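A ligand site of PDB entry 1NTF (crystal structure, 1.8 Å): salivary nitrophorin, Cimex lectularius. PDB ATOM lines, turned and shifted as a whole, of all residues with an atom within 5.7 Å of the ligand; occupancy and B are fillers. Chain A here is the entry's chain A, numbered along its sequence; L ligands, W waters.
Merely in contact with the ligand: Trp 14, Ser 16, His 18, Glu 19, Arg 20, Ala 21, Pro 22, Val 44, Gly 48, Phe 49, Asp 52, Pro 54, Gln 56, Gly 57, Val 61, Phe 64, Asn 78, Ile 80 and Thr 87.
Hydrophobic or aromatic side chains within 4 Å of the ligand: Trp 14, Ala 21, Pro 22, Val 44, Phe 49, Pro 54, Val 61, Phe 64, Ile 80 and Tyr 89.
The nearest printed residue that does not touch the ligand is Val 42 (4.2 Å).
Water W5 lies within hydrogen-bond range of O1 of the ligand (2.7 Å), NZ of Lys 75 (2.8 Å) and OD1 of Asn 78 (3.5 Å).
Water W2 bridges the side-chain amide oxygen (OD1) of Asn 78 (2.8 Å) and an oxygen (O4) of the ligand (2.8 Å).
OH of Tyr 89 sits at hydrogen-bond distance from O2 of the ligand (2.5 Å).
The side-chain sulfur of Cys 60 binds an iron atom (FE1) of the ligand (2.4 Å).
NE2 of Gln 65 lies within hydrogen-bond range of O2 of the ligand (2.9 Å).
The side-chain amino group of Lys 75 is in salt-bridge range of an oxygen (O1) of the ligand.
The side-chain carboxylate (OD2) of Asp 52 is in hydrogen-bond range of the backbone NH (N) of Gln 56, 2.9 Å away.
OD1 of Asp 52 sits at hydrogen-bond distance from N of Gly 57 (3.0 Å).
SG of Cys 60 sits close to NE2 of Gln 56, 3.4 Å away.
The backbone carbonyl oxygen of Thr 87 is in hydrogen-bond range of the backbone NH of Val 42, at 2.9 Å.
The side-chain hydroxyl of Thr 87 lies within hydrogen-bond range of the side-chain amide nitrogen of Asn 78 (2.8 Å).
The guanidinium group (NE) of Arg 20 lies within hydrogen-bond range of the side-chain amide oxygen (OE1) of Gln 56, at 3.2 Å.
The side-chain amide oxygen (OE1) of Gln 65 is in hydrogen-bond range of the side-chain amino group (NZ) of Lys 75 (3.4 Å).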
ATOM      1  N   TRP A  14     -21.439  22.817  12.843  1.00  0.00           N
ATOM      2  CA  TRP A  14     -20.241  22.083  12.633  1.00  0.00           C
ATOM      3  C   TRP A  14     -19.071  22.989  12.865  1.00  0.00           C
ATOM      4  O   TRP A  14     -18.947  24.063  12.221  1.00  0.00           O
ATOM      5  CB  TRP A  14     -20.210  21.640  11.214  1.00  0.00           C
ATOM      6  CG  TRP A  14     -19.172  20.674  10.805  1.00  0.00           C
ATOM      7  CD1 TRP A  14     -18.228  20.011  11.568  1.00  0.00           C
ATOM      8  CD2 TRP A  14     -19.027  20.192   9.496  1.00  0.00           C
ATOM      9  NE1 TRP A  14     -17.481  19.166  10.758  1.00  0.00           N
ATOM     10  CE2 TRP A  14     -17.970  19.245   9.491  1.00  0.00           C
ATOM     11  CE3 TRP A  14     -19.727  20.440   8.298  1.00  0.00           C
ATOM     12  CZ2 TRP A  14     -17.572  18.552   8.302  1.00  0.00           C
ATOM     13  CZ3 TRP A  14     -19.327  19.784   7.142  1.00  0.00           C
ATOM     14  CH2 TRP A  14     -18.270  18.855   7.160  1.00  0.00           C
ATOM     15  N   SER A  16     -16.126  23.312  11.697  1.00  0.00           N
ATOM     16  CA  SER A  16     -15.536  22.770  10.479  1.00  0.00           C
ATOM     17  C   SER A  16     -14.135  23.319  10.191  1.00  0.00           C
ATOM     18  O   SER A  16     -13.463  22.802   9.280  1.00  0.00           O
ATOM     19  CB  SER A  16     -16.433  23.077   9.330  1.00  0.00           C
ATOM     20  OG  SER A  16     -16.574  24.474   9.251  1.00  0.00           O
ATOM     21  N   GLY A  17     -13.679  24.290  10.957  1.00  0.00           N
ATOM     22  CA  GLY A  17     -12.293  24.707  10.887  1.00  0.00           C
ATOM     23  C   GLY A  17     -12.017  25.369   9.534  1.00  0.00           C
ATOM     24  O   GLY A  17     -12.616  26.400   9.191  1.00  0.00           O
ATOM     25  N   HIS A  18     -11.146  24.716   8.738  1.00  0.00           N
ATOM     26  CA  HIS A  18     -10.661  25.235   7.459  1.00  0.00           C
ATOM     27  C   HIS A  18     -11.350  24.501   6.296  1.00  0.00           C
ATOM     28  O   HIS A  18     -11.154  24.806   5.137  1.00  0.00           O
ATOM     29  CB  HIS A  18      -9.097  25.040   7.356  1.00  0.00           C
ATOM     30  CG  HIS A  18      -8.281  26.021   8.176  1.00  0.00           C
ATOM     31  ND1 HIS A  18      -7.636  27.120   7.633  1.00  0.00           N
ATOM     32  CD2 HIS A  18      -7.968  26.037   9.506  1.00  0.00           C
ATOM     33  CE1 HIS A  18      -6.986  27.776   8.586  1.00  0.00           C
ATOM     34  NE2 HIS A  18      -7.165  27.139   9.733  1.00  0.00           N
ATOM     35  N   GLU A  19     -12.199  23.548   6.624  1.00  0.00           N
ATOM     36  CA  GLU A  19     -12.783  22.669   5.642  1.00  0.00           C
ATOM     37  C   GLU A  19     -13.872  23.406   4.850  1.00  0.00           C
ATOM     38  O   GLU A  19     -14.612  24.236   5.398  1.00  0.00           O
ATOM     39  CB  GLU A  19     -13.389  21.470   6.347  1.00  0.00           C
ATOM     40  CG  GLU A  19     -13.695  20.302   5.447  1.00  0.00           C
ATOM     41  CD  GLU A  19     -12.477  19.770   4.715  1.00  0.00           C
ATOM     42  OE1 GLU A  19     -12.733  19.108   3.656  1.00  0.00           O
ATOM     43  OE2 GLU A  19     -11.302  19.996   5.192  1.00  0.00           O
ATOM     44  N   ARG A  20     -13.969  23.039   3.554  1.00  0.00           N
ATOM     45  CA  ARG A  20     -14.976  23.618   2.669  1.00  0.00           C
ATOM     46  C   ARG A  20     -16.278  22.829   2.776  1.00  0.00           C
ATOM     47  O   ARG A  20     -16.291  21.646   3.132  1.00  0.00           O
ATOM     48  CB  ARG A  20     -14.493  23.734   1.200  1.00  0.00           C
ATOM     49  CG  ARG A  20     -13.616  22.554   0.634  1.00  0.00           C
ATOM     50  CD  ARG A  20     -12.896  22.814  -0.732  1.00  0.00           C
ATOM     51  NE  ARG A  20     -12.854  24.235  -1.175  1.00  0.00           N
ATOM     52  CZ  ARG A  20     -11.916  25.158  -0.859  1.00  0.00           C
ATOM     53  NH1 ARG A  20     -10.907  24.868  -0.046  1.00  0.00           N
ATOM     54  NH2 ARG A  20     -12.015  26.394  -1.365  1.00  0.00           N
ATOM     55  N   ALA A  21     -17.385  23.499   2.460  1.00  0.00           N
ATOM     56  CA  ALA A  21     -18.700  22.862   2.359  1.00  0.00           C
ATOM     57  C   ALA A  21     -18.605  21.580   1.523  1.00  0.00           C
ATOM     58  O   ALA A  21     -18.069  21.605   0.409  1.00  0.00           O
ATOM     59  CB  ALA A  21     -19.734  23.887   1.769  1.00  0.00           C
ATOM     60  N   PRO A  22     -19.149  20.468   2.028  1.00  0.00           N
ATOM     61  CA  PRO A  22     -19.124  19.213   1.262  1.00  0.00           C
ATOM     62  C   PRO A  22     -20.097  19.286   0.088  1.00  0.00           C
ATOM     63  O   PRO A  22     -20.827  20.265  -0.044  1.00  0.00           O
ATOM     64  CB  PRO A  22     -19.609  18.150   2.246  1.00  0.00           C
ATOM     65  CG  PRO A  22     -20.408  18.907   3.257  1.00  0.00           C
ATOM     66  CD  PRO A  22     -19.888  20.330   3.284  1.00  0.00           C
ATOM     67  N   LEU A  28     -26.557  16.553   5.225  1.00  0.00           N
ATOM     68  CA  LEU A  28     -26.118  17.530   6.242  1.00  0.00           C
ATOM     69  C   LEU A  28     -27.330  18.235   6.850  1.00  0.00           C
ATOM     70  O   LEU A  28     -27.367  18.498   8.061  1.00  0.00           O
ATOM     71  CB  LEU A  28     -25.243  18.582   5.613  1.00  0.00           C
ATOM     72  CG  LEU A  28     -24.464  19.504   6.536  1.00  0.00           C
ATOM     73  CD1 LEU A  28     -23.483  18.705   7.418  1.00  0.00           C
ATOM     74  CD2 LEU A  28     -23.721  20.621   5.758  1.00  0.00           C
ATOM     75  N   VAL A  42     -28.129  26.890   9.963  1.00  0.00           N
ATOM     76  CA  VAL A  42     -26.823  26.303   9.822  1.00  0.00           C
ATOM     77  C   VAL A  42     -25.797  27.195  10.480  1.00  0.00           C
ATOM     78  O   VAL A  42     -25.724  28.397  10.198  1.00  0.00           O
ATOM     79  CB  VAL A  42     -26.462  26.213   8.268  1.00  0.00           C
ATOM     80  CG1 VAL A  42     -25.163  25.466   8.021  1.00  0.00           C
ATOM     81  CG2 VAL A  42     -27.634  25.489   7.531  1.00  0.00           C
ATOM     82  N   VAL A  44     -21.709  27.431  11.516  1.00  0.00           N
ATOM     83  CA  VAL A  44     -20.367  26.919  11.404  1.00  0.00           C
ATOM     84  C   VAL A  44     -19.373  27.716  12.232  1.00  0.00           C
ATOM     85  O   VAL A  44     -19.578  28.929  12.525  1.00  0.00           O
ATOM     86  CB  VAL A  44     -19.840  26.819   9.945  1.00  0.00           C
ATOM     87  CG1 VAL A  44     -20.477  25.710   9.180  1.00  0.00           C
ATOM     88  CG2 VAL A  44     -19.936  28.165   9.250  1.00  0.00           C
ATOM     89  N   PHE A  47     -12.136  29.318  10.712  1.00  0.00           N
ATOM     90  CA  PHE A  47     -11.094  30.373  10.541  1.00  0.00           C
ATOM     91  C   PHE A  47     -11.181  30.991   9.161  1.00  0.00           C
ATOM     92  O   PHE A  47     -11.323  30.271   8.201  1.00  0.00           O
ATOM     93  CB  PHE A  47      -9.688  29.774  10.755  1.00  0.00           C
ATOM     94  CG  PHE A  47      -9.527  29.039  12.046  1.00  0.00           C
ATOM     95  CD1 PHE A  47      -9.556  27.637  12.078  1.00  0.00           C
ATOM     96  CD2 PHE A  47      -9.383  29.744  13.257  1.00  0.00           C
ATOM     97  CE1 PHE A  47      -9.411  26.930  13.311  1.00  0.00           C
ATOM     98  CE2 PHE A  47      -9.247  29.055  14.501  1.00  0.00           C
ATOM     99  CZ  PHE A  47      -9.266  27.654  14.524  1.00  0.00           C
ATOM    100  N   GLY A  48     -11.126  32.316   9.072  1.00  0.00           N
ATOM    101  CA  GLY A  48     -10.989  33.010   7.788  1.00  0.00           C
ATOM    102  C   GLY A  48     -12.180  33.084   6.847  1.00  0.00           C
ATOM    103  O   GLY A  48     -11.986  33.184   5.617  1.00  0.00           O
ATOM    104  N   PHE A  49     -13.404  33.012   7.378  1.00  0.00           N
ATOM    105  CA  PHE A  49     -14.571  33.016   6.512  1.00  0.00           C
ATOM    106  C   PHE A  49     -14.707  34.357   5.784  1.00  0.00           C
ATOM    107  O   PHE A  49     -15.021  34.378   4.588  1.00  0.00           O
ATOM    108  CB  PHE A  49     -15.834  32.799   7.309  1.00  0.00           C
ATOM    109  CG  PHE A  49     -15.927  31.466   8.000  1.00  0.00           C
ATOM    110  CD1 PHE A  49     -16.381  31.407   9.295  1.00  0.00           C
ATOM    111  CD2 PHE A  49     -15.660  30.285   7.351  1.00  0.00           C
ATOM    112  CE1 PHE A  49     -16.564  30.199   9.913  1.00  0.00           C
ATOM    113  CE2 PHE A  49     -15.816  29.043   7.987  1.00  0.00           C
ATOM    114  CZ  PHE A  49     -16.247  29.004   9.265  1.00  0.00           C
ATOM    115  N   GLN A  50     -14.490  35.468   6.514  1.00  0.00           N
ATOM    116  CA  GLN A  50     -14.599  36.821   5.949  1.00  0.00           C
ATOM    117  C   GLN A  50     -13.487  37.100   4.941  1.00  0.00           C
ATOM    118  O   GLN A  50     -13.741  37.267   3.752  1.00  0.00           O
ATOM    119  CB  GLN A  50     -14.628  37.880   7.057  1.00  0.00           C
ATOM    120  CG  GLN A  50     -15.888  38.775   7.019  1.00  0.00           C
ATOM    121  CD  GLN A  50     -15.839  39.915   8.068  1.00  0.00           C
ATOM    122  OE1 GLN A  50     -15.292  39.746   9.177  1.00  0.00           O
ATOM    123  NE2 GLN A  50     -16.410  41.067   7.708  1.00  0.00           N
ATOM    124  N   ASP A  52     -11.856  35.102   3.387  1.00  0.00           N
ATOM    125  CA  ASP A  52     -12.064  34.126   2.318  1.00  0.00           C
ATOM    126  C   ASP A  52     -10.870  34.003   1.344  1.00  0.00           C
ATOM    127  O   ASP A  52     -11.047  34.107   0.121  1.00  0.00           O
ATOM    128  CB  ASP A  52     -13.351  34.461   1.540  1.00  0.00           C
ATOM    129  CG  ASP A  52     -13.871  33.286   0.752  1.00  0.00           C
ATOM    130  OD1 ASP A  52     -14.849  33.460  -0.020  1.00  0.00           O
ATOM    131  OD2 ASP A  52     -13.372  32.139   0.809  1.00  0.00           O
ATOM    132  N   LYS A  53      -9.658  33.769   1.858  1.00  0.00           N
ATOM    133  CA  LYS A  53      -8.506  33.520   0.960  1.00  0.00           C
ATOM    134  C   LYS A  53      -8.818  32.472  -0.129  1.00  0.00           C
ATOM    135  O   LYS A  53      -8.612  32.768  -1.310  1.00  0.00           O
ATOM    136  CB  LYS A  53      -7.223  33.116   1.721  1.00  0.00           C
ATOM    137  CG  LYS A  53      -6.553  34.271   2.502  1.00  0.00           C
ATOM    138  CD  LYS A  53      -5.427  34.982   1.698  1.00  0.00           C
ATOM    139  CE  LYS A  53      -4.952  36.313   2.369  1.00  0.00           C
ATOM    140  NZ  LYS A  53      -3.592  36.766   1.869  1.00  0.00           N
ATOM    141  N   PRO A  54      -9.324  31.269   0.247  1.00  0.00           N
ATOM    142  CA  PRO A  54      -9.631  30.200  -0.734  1.00  0.00           C
ATOM    143  C   PRO A  54     -10.787  30.459  -1.736  1.00  0.00           C
ATOM    144  O   PRO A  54     -10.955  29.677  -2.663  1.00  0.00           O
ATOM    145  CB  PRO A  54     -10.032  29.000   0.149  1.00  0.00           C
ATOM    146  CG  PRO A  54     -10.266  29.522   1.519  1.00  0.00           C
ATOM    147  CD  PRO A  54      -9.595  30.846   1.633  1.00  0.00           C
ATOM    148  N   GLN A  56     -14.094  30.252  -1.283  1.00  0.00           N
ATOM    149  CA  GLN A  56     -15.162  29.257  -1.088  1.00  0.00           C
ATOM    150  C   GLN A  56     -16.563  29.892  -1.066  1.00  0.00           C
ATOM    151  O   GLN A  56     -17.542  29.235  -1.387  1.00  0.00           O
ATOM    152  CB  GLN A  56     -14.941  28.534   0.247  1.00  0.00           C
ATOM    153  CG  GLN A  56     -16.083  27.598   0.697  1.00  0.00           C
ATOM    154  CD  GLN A  56     -16.295  26.460  -0.267  1.00  0.00           C
ATOM    155  OE1 GLN A  56     -15.402  26.128  -1.071  1.00  0.00           O
ATOM    156  NE2 GLN A  56     -17.490  25.873  -0.247  1.00  0.00           N
ATOM    157  N   GLY A  57     -16.651  31.120  -0.597  1.00  0.00           N
ATOM    158  CA  GLY A  57     -17.925  31.846  -0.552  1.00  0.00           C
ATOM    159  C   GLY A  57     -18.838  31.626  -1.763  1.00  0.00           C
ATOM    160  O   GLY A  57     -19.963  31.232  -1.601  1.00  0.00           O
ATOM    161  N   PRO A  58     -18.362  31.888  -2.987  1.00  0.00           N
ATOM    162  CA  PRO A  58     -19.193  31.700  -4.171  1.00  0.00           C
ATOM    163  C   PRO A  58     -19.637  30.288  -4.356  1.00  0.00           C
ATOM    164  O   PRO A  58     -20.726  30.131  -4.874  1.00  0.00           O
ATOM    165  CB  PRO A  58     -18.294  32.151  -5.341  1.00  0.00           C
ATOM    166  CG  PRO A  58     -17.134  32.772  -4.776  1.00  0.00           C
ATOM    167  CD  PRO A  58     -17.031  32.426  -3.308  1.00  0.00           C
ATOM    168  N   CYS A  60     -20.321  28.060  -1.774  1.00  0.00           N
ATOM    169  CA  CYS A  60     -21.355  27.905  -0.741  1.00  0.00           C
ATOM    170  C   CYS A  60     -22.709  28.408  -1.234  1.00  0.00           C
ATOM    171  O   CYS A  60     -23.714  27.677  -1.211  1.00  0.00           O
ATOM    172  CB  CYS A  60     -20.973  28.721   0.499  1.00  0.00           C
ATOM    173  SG  CYS A  60     -19.621  27.934   1.416  1.00  0.00           S
ATOM    174  N   VAL A  61     -22.658  29.635  -1.755  1.00  0.00           N
ATOM    175  CA  VAL A  61     -23.860  30.317  -2.224  1.00  0.00           C
ATOM    176  C   VAL A  61     -24.470  29.458  -3.296  1.00  0.00           C
ATOM    177  O   VAL A  61     -25.598  29.025  -3.148  1.00  0.00           O
ATOM    178  CB  VAL A  61     -23.586  31.703  -2.772  1.00  0.00           C
ATOM    179  CG1 VAL A  61     -24.890  32.329  -3.321  1.00  0.00           C
ATOM    180  CG2 VAL A  61     -23.003  32.604  -1.698  1.00  0.00           C
ATOM    181  N   PHE A  64     -25.740  25.797  -1.902  1.00  0.00           N
ATOM    182  CA  PHE A  64     -26.865  25.881  -0.989  1.00  0.00           C
ATOM    183  C   PHE A  64     -28.086  26.478  -1.699  1.00  0.00           C
ATOM    184  O   PHE A  64     -29.211  25.925  -1.563  1.00  0.00           O
ATOM    185  CB  PHE A  64     -26.502  26.701   0.241  1.00  0.00           C
ATOM    186  CG  PHE A  64     -25.755  25.931   1.288  1.00  0.00           C
ATOM    187  CD1 PHE A  64     -24.340  25.954   1.312  1.00  0.00           C
ATOM    188  CD2 PHE A  64     -26.459  25.149   2.221  1.00  0.00           C
ATOM    189  CE1 PHE A  64     -23.619  25.203   2.290  1.00  0.00           C
ATOM    190  CE2 PHE A  64     -25.768  24.399   3.209  1.00  0.00           C
ATOM    191  CZ  PHE A  64     -24.353  24.439   3.264  1.00  0.00           C
ATOM    192  N   GLN A  65     -27.857  27.557  -2.469  1.00  0.00           N
ATOM    193  CA  GLN A  65     -28.980  28.275  -3.144  1.00  0.00           C
ATOM    194  C   GLN A  65     -29.645  27.375  -4.171  1.00  0.00           C
ATOM    195  O   GLN A  65     -30.864  27.288  -4.194  1.00  0.00           O
ATOM    196  CB  GLN A  65     -28.546  29.662  -3.706  1.00  0.00           C
ATOM    197  CG  GLN A  65     -29.479  30.839  -3.272  1.00  0.00           C
ATOM    198  CD  GLN A  65     -29.209  31.423  -1.848  1.00  0.00           C
ATOM    199  OE1 GLN A  65     -28.462  32.425  -1.692  1.00  0.00           O
ATOM    200  NE2 GLN A  65     -29.852  30.831  -0.833  1.00  0.00           N
ATOM    201  N   LEU A  68     -31.669  24.528  -2.151  1.00  0.00           N
ATOM    202  CA  LEU A  68     -32.766  24.976  -1.272  1.00  0.00           C
ATOM    203  C   LEU A  68     -33.852  25.777  -1.997  1.00  0.00           C
ATOM    204  O   LEU A  68     -35.046  25.616  -1.704  1.00  0.00           O
ATOM    205  CB  LEU A  68     -32.208  25.725  -0.072  1.00  0.00           C
ATOM    206  CG  LEU A  68     -31.431  24.768   0.908  1.00  0.00           C
ATOM    207  CD1 LEU A  68     -30.548  25.595   1.815  1.00  0.00           C
ATOM    208  CD2 LEU A  68     -32.379  23.901   1.753  1.00  0.00           C
ATOM    209  N   LYS A  75     -33.629  32.381   1.695  1.00  0.00           N
ATOM    210  CA  LYS A  75     -32.664  32.722   2.769  1.00  0.00           C
ATOM    211  C   LYS A  75     -33.086  34.001   3.453  1.00  0.00           C
ATOM    212  O   LYS A  75     -33.205  35.048   2.837  1.00  0.00           O
ATOM    213  CB  LYS A  75     -31.274  32.866   2.211  1.00  0.00           C
ATOM    214  CG  LYS A  75     -30.246  33.468   3.151  1.00  0.00           C
ATOM    215  CD  LYS A  75     -28.888  33.427   2.553  1.00  0.00           C
ATOM    216  CE  LYS A  75     -28.726  34.563   1.464  1.00  0.00           C
ATOM    217  NZ  LYS A  75     -27.367  34.499   0.793  1.00  0.00           N
ATOM    218  N   ASN A  78     -27.724  35.435   5.950  1.00  0.00           N
ATOM    219  CA  ASN A  78     -26.418  34.833   6.159  1.00  0.00           C
ATOM    220  C   ASN A  78     -25.583  35.869   6.814  1.00  0.00           C
ATOM    221  O   ASN A  78     -25.558  37.041   6.367  1.00  0.00           O
ATOM    222  CB  ASN A  78     -25.748  34.404   4.865  1.00  0.00           C
ATOM    223  CG  ASN A  78     -24.270  33.974   5.057  1.00  0.00           C
ATOM    224  OD1 ASN A  78     -23.375  34.715   4.700  1.00  0.00           O
ATOM    225  ND2 ASN A  78     -24.038  32.810   5.655  1.00  0.00           N
ATOM    226  N   ILE A  80     -21.600  36.293   8.458  1.00  0.00           N
ATOM    227  CA  ILE A  80     -20.296  35.696   8.719  1.00  0.00           C
ATOM    228  C   ILE A  80     -19.353  36.694   9.384  1.00  0.00           C
ATOM    229  O   ILE A  80     -19.442  37.893   9.136  1.00  0.00           O
ATOM    230  CB  ILE A  80     -19.656  35.144   7.471  1.00  0.00           C
ATOM    231  CG1 ILE A  80     -19.517  36.248   6.418  1.00  0.00           C
ATOM    232  CG2 ILE A  80     -20.509  34.014   6.857  1.00  0.00           C
ATOM    233  CD1 ILE A  80     -18.662  35.794   5.248  1.00  0.00           C
ATOM    234  N   THR A  87     -26.575  30.940   9.019  1.00  0.00           N
ATOM    235  CA  THR A  87     -27.599  31.053   7.978  1.00  0.00           C
ATOM    236  C   THR A  87     -28.922  30.526   8.391  1.00  0.00           C
ATOM    237  O   THR A  87     -29.005  29.452   9.006  1.00  0.00           O
ATOM    238  CB  THR A  87     -27.155  30.282   6.732  1.00  0.00           C
ATOM    239  OG1 THR A  87     -25.809  30.740   6.383  1.00  0.00           O
ATOM    240  CG2 THR A  87     -28.005  30.679   5.553  1.00  0.00           C
ATOM    241  N   TYR A  89     -32.808  29.787   6.810  1.00  0.00           N
ATOM    242  CA  TYR A  89     -33.708  29.630   5.666  1.00  0.00           C
ATOM    243  C   TYR A  89     -35.116  29.361   6.171  1.00  0.00           C
ATOM    244  O   TYR A  89     -35.316  28.640   7.169  1.00  0.00           O
ATOM    245  CB  TYR A  89     -33.261  28.480   4.785  1.00  0.00           C
ATOM    246  CG  TYR A  89     -31.896  28.547   4.207  1.00  0.00           C
ATOM    247  CD1 TYR A  89     -30.804  27.944   4.872  1.00  0.00           C
ATOM    248  CD2 TYR A  89     -31.624  29.194   3.004  1.00  0.00           C
ATOM    249  CE1 TYR A  89     -29.521  27.992   4.340  1.00  0.00           C
ATOM    250  CE2 TYR A  89     -30.353  29.232   2.481  1.00  0.00           C
ATOM    251  CZ  TYR A  89     -29.292  28.627   3.174  1.00  0.00           C
ATOM    252  OH  TYR A  89     -28.012  28.676   2.742  1.00  0.00           O
HETATM  253  C1  LIG L   1     -21.788  31.365   2.800  1.00  0.00           C
HETATM  254  C2  LIG L   1     -22.056  27.025   4.968  1.00  0.00           C
HETATM  255  C3  LIG L   1     -17.262  26.762   4.684  1.00  0.00           C
HETATM  256  C4  LIG L   1     -16.919  31.328   3.224  1.00  0.00           C
HETATM  257  C5  LIG L   1     -22.296  30.224   3.363  1.00  0.00           C
HETATM  258  C6  LIG L   1     -23.698  29.873   3.489  1.00  0.00           C
HETATM  259  C7  LIG L   1     -23.781  28.658   4.101  1.00  0.00           C
HETATM  260  C8  LIG L   1     -22.435  28.229   4.369  1.00  0.00           C
HETATM  261  C9  LIG L   1     -25.014  27.842   4.529  1.00  0.00           C
HETATM  262  C10 LIG L   1     -24.834  30.759   2.942  1.00  0.00           C
HETATM  263  C11 LIG L   1     -25.182  30.199   1.537  1.00  0.00           C
HETATM  264  C12 LIG L   1     -26.390  30.878   0.896  1.00  0.00           C
HETATM  265  O1  LIG L   1     -26.167  31.999   0.411  1.00  0.00           O
HETATM  266  O2  LIG L   1     -27.512  30.293   0.848  1.00  0.00           O
HETATM  267  C13 LIG L   1     -20.789  26.521   5.025  1.00  0.00           C
HETATM  268  C14 LIG L   1     -20.364  25.221   5.557  1.00  0.00           C
HETATM  269  C15 LIG L   1     -19.009  25.208   5.474  1.00  0.00           C
HETATM  270  C16 LIG L   1     -18.555  26.444   4.908  1.00  0.00           C
HETATM  271  C17 LIG L   1     -21.338  24.153   6.100  1.00  0.00           C
HETATM  272  C18 LIG L   1     -17.981  24.154   5.860  1.00  0.00           C
HETATM  273  C19 LIG L   1     -18.326  22.874   5.692  1.00  0.00           C
HETATM  274  C20 LIG L   1     -16.706  27.978   4.341  1.00  0.00           C
HETATM  275  C21 LIG L   1     -15.296  28.331   4.297  1.00  0.00           C
HETATM  276  C22 LIG L   1     -15.234  29.607   3.891  1.00  0.00           C
HETATM  277  C23 LIG L   1     -16.569  30.063   3.656  1.00  0.00           C
HETATM  278  C24 LIG L   1     -14.096  27.412   4.622  1.00  0.00           C
HETATM  279  C25 LIG L   1     -14.038  30.541   3.624  1.00  0.00           C
HETATM  280  C26 LIG L   1     -12.814  30.327   4.130  1.00  0.00           C
HETATM  281  C27 LIG L   1     -18.184  31.790   2.983  1.00  0.00           C
HETATM  282  C28 LIG L   1     -18.509  33.124   2.549  1.00  0.00           C
HETATM  283  C29 LIG L   1     -20.030  33.119   2.413  1.00  0.00           C
HETATM  284  C30 LIG L   1     -20.474  31.802   2.790  1.00  0.00           C
HETATM  285  C31 LIG L   1     -17.538  34.283   2.295  1.00  0.00           C
HETATM  286  C32 LIG L   1     -20.864  34.353   2.021  1.00  0.00           C
HETATM  287  C33 LIG L   1     -20.735  34.574   0.539  1.00  0.00           C
HETATM  288  C34 LIG L   1     -21.529  35.798   0.117  1.00  0.00           C
HETATM  289  O3  LIG L   1     -21.223  36.264  -1.022  1.00  0.00           O
HETATM  290  O4  LIG L   1     -22.432  36.273   0.895  1.00  0.00           O
HETATM  291  N1  LIG L   1     -21.571  29.188   3.871  1.00  0.00           N
HETATM  292  N2  LIG L   1     -19.648  27.205   4.681  1.00  0.00           N
HETATM  293  N3  LIG L   1     -17.443  29.025   3.935  1.00  0.00           N
HETATM  294  N4  LIG L   1     -19.351  31.070   3.111  1.00  0.00           N
HETATM  295 FE1  LIG L   1     -19.529  29.010   3.576  1.00  0.00          FE
HETATM  296  O   HOH W   1     -18.155  35.309  -1.879  1.00  0.00           O
HETATM  297  O   HOH W   2     -23.227  37.167   3.458  1.00  0.00           O
HETATM  298  O   HOH W   3     -19.303  29.910   6.196  1.00  0.00           O
HETATM  299  O   HOH W   4     -21.748  30.552   6.653  1.00  0.00           O
HETATM  300  O   HOH W   5     -24.749  33.989   1.613  1.00  0.00           O
